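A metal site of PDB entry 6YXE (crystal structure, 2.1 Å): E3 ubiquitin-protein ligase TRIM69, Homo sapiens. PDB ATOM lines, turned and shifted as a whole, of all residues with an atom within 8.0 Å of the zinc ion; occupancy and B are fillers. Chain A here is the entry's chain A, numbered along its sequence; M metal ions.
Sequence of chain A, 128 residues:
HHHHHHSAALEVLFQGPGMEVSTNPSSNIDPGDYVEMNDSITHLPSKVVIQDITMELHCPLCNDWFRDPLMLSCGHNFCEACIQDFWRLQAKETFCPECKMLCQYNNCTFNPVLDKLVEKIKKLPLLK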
ATOM      1  N   HIS A  58     -25.134 -23.045  -7.863  1.00  0.00           N
ATOM      2  CA  HIS A  58     -25.772 -22.875  -6.540  1.00  0.00           C
ATOM      3  C   HIS A  58     -25.015 -23.661  -5.489  1.00  0.00           C
ATOM      4  O   HIS A  58     -24.654 -24.804  -5.683  1.00  0.00           O
ATOM      5  CB  HIS A  58     -27.235 -23.328  -6.558  1.00  0.00           C
ATOM      6  CG  HIS A  58     -28.163 -22.265  -7.075  1.00  0.00           C
ATOM      7  ND1 HIS A  58     -28.119 -21.833  -8.380  1.00  0.00           N
ATOM      8  CD2 HIS A  58     -29.152 -21.561  -6.456  1.00  0.00           C
ATOM      9  CE1 HIS A  58     -29.013 -20.870  -8.530  1.00  0.00           C
ATOM     10  NE2 HIS A  58     -29.659 -20.680  -7.385  1.00  0.00           N
ATOM     11  N   CYS A  59     -24.765 -22.987  -4.358  1.00  0.00           N
ATOM     12  CA  CYS A  59     -24.127 -23.586  -3.203  1.00  0.00           C
ATOM     13  C   CYS A  59     -25.071 -24.623  -2.560  1.00  0.00           C
ATOM     14  O   CYS A  59     -26.219 -24.300  -2.275  1.00  0.00           O
ATOM     15  CB  CYS A  59     -23.796 -22.477  -2.208  1.00  0.00           C
ATOM     16  SG  CYS A  59     -23.215 -23.023  -0.594  1.00  0.00           S
ATOM     17  N   PRO A  60     -24.584 -25.863  -2.341  1.00  0.00           N
ATOM     18  CA  PRO A  60     -25.490 -26.838  -1.696  1.00  0.00           C
ATOM     19  C   PRO A  60     -25.794 -26.591  -0.230  1.00  0.00           C
ATOM     20  O   PRO A  60     -26.733 -27.174   0.278  1.00  0.00           O
ATOM     21  CB  PRO A  60     -24.766 -28.190  -1.867  1.00  0.00           C
ATOM     22  CG  PRO A  60     -23.600 -27.906  -2.759  1.00  0.00           C
ATOM     23  CD  PRO A  60     -23.281 -26.444  -2.667  1.00  0.00           C
ATOM     24  N   LEU A  61     -25.016 -25.794   0.460  1.00  0.00           N
ATOM     25  CA  LEU A  61     -25.304 -25.485   1.876  1.00  0.00           C
ATOM     26  C   LEU A  61     -26.433 -24.471   2.014  1.00  0.00           C
ATOM     27  O   LEU A  61     -27.337 -24.709   2.773  1.00  0.00           O
ATOM     28  CB  LEU A  61     -24.044 -25.025   2.617  1.00  0.00           C
ATOM     29  CG  LEU A  61     -23.102 -26.170   3.029  1.00  0.00           C
ATOM     30  CD1 LEU A  61     -21.795 -25.598   3.566  1.00  0.00           C
ATOM     31  CD2 LEU A  61     -23.763 -27.113   4.010  1.00  0.00           C
ATOM     32  N   CYS A  62     -26.388 -23.365   1.260  1.00  0.00           N
ATOM     33  CA  CYS A  62     -27.428 -22.325   1.376  1.00  0.00           C
ATOM     34  C   CYS A  62     -28.483 -22.382   0.272  1.00  0.00           C
ATOM     35  O   CYS A  62     -29.519 -21.710   0.422  1.00  0.00           O
ATOM     36  CB  CYS A  62     -26.820 -20.915   1.404  1.00  0.00           C
ATOM     37  SG  CYS A  62     -25.957 -20.458  -0.114  1.00  0.00           S
ATOM     38  N   ASN A  63     -28.235 -23.133  -0.802  1.00  0.00           N
ATOM     39  CA  ASN A  63     -29.172 -23.244  -1.938  1.00  0.00           C
ATOM     40  C   ASN A  63     -29.403 -21.893  -2.668  1.00  0.00           C
ATOM     41  O   ASN A  63     -30.429 -21.667  -3.291  1.00  0.00           O
ATOM     42  CB  ASN A  63     -30.521 -23.876  -1.519  1.00  0.00           C
ATOM     43  CG  ASN A  63     -30.374 -25.347  -1.075  1.00  0.00           C
ATOM     44  OD1 ASN A  63     -29.763 -26.153  -1.757  1.00  0.00           O
ATOM     45  ND2 ASN A  63     -30.945 -25.673   0.086  1.00  0.00           N
ATOM     46  N   ASP A  64     -28.418 -20.991  -2.559  1.00  0.00           N
ATOM     47  CA  ASP A  64     -28.401 -19.732  -3.268  1.00  0.00           C
ATOM     48  C   ASP A  64     -27.190 -19.722  -4.164  1.00  0.00           C
ATOM     49  O   ASP A  64     -26.400 -20.677  -4.109  1.00  0.00           O
ATOM     50  CB  ASP A  64     -28.300 -18.546  -2.258  1.00  0.00           C
ATOM     51  CG  ASP A  64     -28.951 -17.306  -2.759  1.00  0.00           C
ATOM     52  OD1 ASP A  64     -29.302 -17.174  -3.968  1.00  0.00           O
ATOM     53  OD2 ASP A  64     -29.079 -16.419  -1.956  1.00  0.00           O
ATOM     54  N   TRP A  65     -27.048 -18.685  -4.995  1.00  0.00           N
ATOM     55  CA  TRP A  65     -25.899 -18.537  -5.872  1.00  0.00           C
ATOM     56  C   TRP A  65     -24.621 -18.554  -5.081  1.00  0.00           C
ATOM     57  O   TRP A  65     -24.557 -17.934  -4.043  1.00  0.00           O
ATOM     58  CB  TRP A  65     -25.957 -17.187  -6.607  1.00  0.00           C
ATOM     59  CG  TRP A  65     -27.198 -17.034  -7.517  1.00  0.00           C
ATOM     60  CD1 TRP A  65     -28.298 -16.316  -7.258  1.00  0.00           C
ATOM     61  CD2 TRP A  65     -27.387 -17.623  -8.795  1.00  0.00           C
ATOM     62  NE1 TRP A  65     -29.185 -16.414  -8.290  1.00  0.00           N
ATOM     63  CE2 TRP A  65     -28.650 -17.227  -9.253  1.00  0.00           C
ATOM     64  CE3 TRP A  65     -26.621 -18.499  -9.576  1.00  0.00           C
ATOM     65  CZ2 TRP A  65     -29.158 -17.643 -10.490  1.00  0.00           C
ATOM     66  CZ3 TRP A  65     -27.149 -18.921 -10.807  1.00  0.00           C
ATOM     67  CH2 TRP A  65     -28.406 -18.479 -11.242  1.00  0.00           C
ATOM     68  N   PHE A  66     -23.573 -19.212  -5.566  1.00  0.00           N
ATOM     69  CA  PHE A  66     -22.259 -19.088  -4.908  1.00  0.00           C
ATOM     70  C   PHE A  66     -21.907 -17.634  -4.697  1.00  0.00           C
ATOM     71  O   PHE A  66     -22.076 -16.825  -5.612  1.00  0.00           O
ATOM     72  CB  PHE A  66     -21.145 -19.710  -5.755  1.00  0.00           C
ATOM     73  CG  PHE A  66     -21.164 -21.192  -5.772  1.00  0.00           C
ATOM     74  CD1 PHE A  66     -21.011 -21.925  -4.588  1.00  0.00           C
ATOM     75  CD2 PHE A  66     -21.313 -21.873  -6.965  1.00  0.00           C
ATOM     76  CE1 PHE A  66     -21.045 -23.289  -4.618  1.00  0.00           C
ATOM     77  CE2 PHE A  66     -21.330 -23.250  -6.986  1.00  0.00           C
ATOM     78  CZ  PHE A  66     -21.217 -23.962  -5.812  1.00  0.00           C
ATOM     79  N   ARG A  67     -21.440 -17.306  -3.482  1.00  0.00           N
ATOM     80  CA  ARG A  67     -20.841 -16.009  -3.168  1.00  0.00           C
ATOM     81  C   ARG A  67     -19.466 -16.256  -2.517  1.00  0.00           C
ATOM     82  O   ARG A  67     -19.371 -16.964  -1.513  1.00  0.00           O
ATOM     83  CB  ARG A  67     -21.735 -15.206  -2.219  1.00  0.00           C
ATOM     84  N   PRO A  69     -17.032 -18.373  -3.472  1.00  0.00           N
ATOM     85  CA  PRO A  69     -16.943 -19.793  -3.281  1.00  0.00           C
ATOM     86  C   PRO A  69     -15.514 -20.217  -3.022  1.00  0.00           C
ATOM     87  O   PRO A  69     -14.588 -19.651  -3.615  1.00  0.00           O
ATOM     88  CB  PRO A  69     -17.478 -20.386  -4.602  1.00  0.00           C
ATOM     89  CG  PRO A  69     -17.338 -19.313  -5.596  1.00  0.00           C
ATOM     90  CD  PRO A  69     -17.502 -18.045  -4.817  1.00  0.00           C
ATOM     91  N   ASN A  77     -17.405 -27.159  -4.047  1.00  0.00           N
ATOM     92  CA  ASN A  77     -17.426 -25.713  -3.862  1.00  0.00           C
ATOM     93  C   ASN A  77     -18.594 -25.335  -2.955  1.00  0.00           C
ATOM     94  O   ASN A  77     -19.672 -25.929  -3.053  1.00  0.00           O
ATOM     95  CB  ASN A  77     -17.624 -24.989  -5.202  1.00  0.00           C
ATOM     96  CG  ASN A  77     -16.459 -25.207  -6.157  1.00  0.00           C
ATOM     97  OD1 ASN A  77     -15.371 -24.656  -5.970  1.00  0.00           O
ATOM     98  ND2 ASN A  77     -16.663 -26.071  -7.141  1.00  0.00           N
ATOM     99  N   PHE A  78     -18.365 -24.346  -2.094  1.00  0.00           N
ATOM    100  CA  PHE A  78     -19.382 -23.772  -1.187  1.00  0.00           C
ATOM    101  C   PHE A  78     -19.063 -22.302  -0.996  1.00  0.00           C
ATOM    102  O   PHE A  78     -17.876 -21.955  -1.022  1.00  0.00           O
ATOM    103  CB  PHE A  78     -19.322 -24.449   0.191  1.00  0.00           C
ATOM    104  CG  PHE A  78     -19.430 -25.924   0.108  1.00  0.00           C
ATOM    105  CD1 PHE A  78     -20.667 -26.542   0.134  1.00  0.00           C
ATOM    106  CD2 PHE A  78     -18.295 -26.706  -0.082  1.00  0.00           C
ATOM    107  CE1 PHE A  78     -20.780 -27.921  -0.028  1.00  0.00           C
ATOM    108  CE2 PHE A  78     -18.396 -28.074  -0.240  1.00  0.00           C
ATOM    109  CZ  PHE A  78     -19.643 -28.671  -0.212  1.00  0.00           C
ATOM    110  N   CYS A  79     -20.057 -21.454  -0.733  1.00  0.00           N
ATOM    111  CA  CYS A  79     -19.754 -20.069  -0.336  1.00  0.00           C
ATOM    112  C   CYS A  79     -18.752 -20.106   0.823  1.00  0.00           C
ATOM    113  O   CYS A  79     -18.848 -20.963   1.697  1.00  0.00           O
ATOM    114  CB  CYS A  79     -20.994 -19.270   0.120  1.00  0.00           C
ATOM    115  SG  CYS A  79     -22.467 -19.437  -0.936  1.00  0.00           S
ATOM    116  N   GLU A  80     -17.782 -19.219   0.800  1.00  0.00           N
ATOM    117  CA  GLU A  80     -16.819 -19.130   1.899  1.00  0.00           C
ATOM    118  C   GLU A  80     -17.503 -19.099   3.255  1.00  0.00           C
ATOM    119  O   GLU A  80     -17.133 -19.870   4.143  1.00  0.00           O
ATOM    120  CB  GLU A  80     -15.938 -17.895   1.716  1.00  0.00           C
ATOM    121  CG  GLU A  80     -14.990 -17.613   2.855  1.00  0.00           C
ATOM    122  CD  GLU A  80     -14.246 -16.288   2.739  1.00  0.00           C
ATOM    123  OE1 GLU A  80     -14.673 -15.390   2.007  1.00  0.00           O
ATOM    124  OE2 GLU A  80     -13.235 -16.158   3.417  1.00  0.00           O
ATOM    125  N   ALA A  81     -18.484 -18.215   3.432  1.00  0.00           N
ATOM    126  CA  ALA A  81     -19.224 -18.051   4.685  1.00  0.00           C
ATOM    127  C   ALA A  81     -19.967 -19.309   5.095  1.00  0.00           C
ATOM    128  O   ALA A  81     -19.997 -19.673   6.272  1.00  0.00           O
ATOM    129  CB  ALA A  81     -20.195 -16.824   4.593  1.00  0.00           C
ATOM    130  N   CYS A  82     -20.508 -20.024   4.102  1.00  0.00           N
ATOM    131  CA  CYS A  82     -21.301 -21.224   4.333  1.00  0.00           C
ATOM    132  C   CYS A  82     -20.440 -22.352   4.865  1.00  0.00           C
ATOM    133  O   CYS A  82     -20.758 -22.965   5.874  1.00  0.00           O
ATOM    134  CB  CYS A  82     -22.014 -21.664   3.051  1.00  0.00           C
ATOM    135  SG  CYS A  82     -23.354 -20.594   2.512  1.00  0.00           S
ATOM    136  N   ILE A  83     -19.322 -22.629   4.210  1.00  0.00           N
ATOM    137  CA  ILE A  83     -18.480 -23.743   4.641  1.00  0.00           C
ATOM    138  C   ILE A  83     -17.767 -23.408   5.974  1.00  0.00           C
ATOM    139  O   ILE A  83     -17.655 -24.264   6.849  1.00  0.00           O
ATOM    140  CB  ILE A  83     -17.513 -24.261   3.537  1.00  0.00           C
ATOM    141  CG1 ILE A  83     -16.858 -25.569   3.949  1.00  0.00           C
ATOM    142  CG2 ILE A  83     -16.403 -23.259   3.247  1.00  0.00           C
ATOM    143  CD1 ILE A  83     -17.835 -26.728   4.014  1.00  0.00           C
HETATM  144 ZN    ZN M   1     -23.739 -20.887   0.316  1.00  0.00          ZN
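Within 4 Å of the zinc ion: Cys 59, Cys 62, Cys 79 and Cys 82.
SG of Cys 82 is bound to the zinc ion, at 2.2 Å.
The zinc ion is bound by SG of Cys 62.
SG of Cys 79 binds the zinc ion, at 2.3 Å.
The zinc ion is bound by SG of Cys 59 (2.4 Å).
The zinc ion has four donor atoms within binding distance.
The side-chain sulfur (SG) of Cys 62 lies close to the backbone NH (N) of Asp 64 (3.5 Å).
The side-chain sulfur of Cys 79 sits close to the backbone NH of Arg 67, at 3.5 Å.
The side-chain sulfur (SG) of Cys 59 lies close to the backbone NH (N) of Leu 61 (3.5 Å).
O of Asp 64 lies within hydrogen-bond range of N of Cys 59 (2.8 Å).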
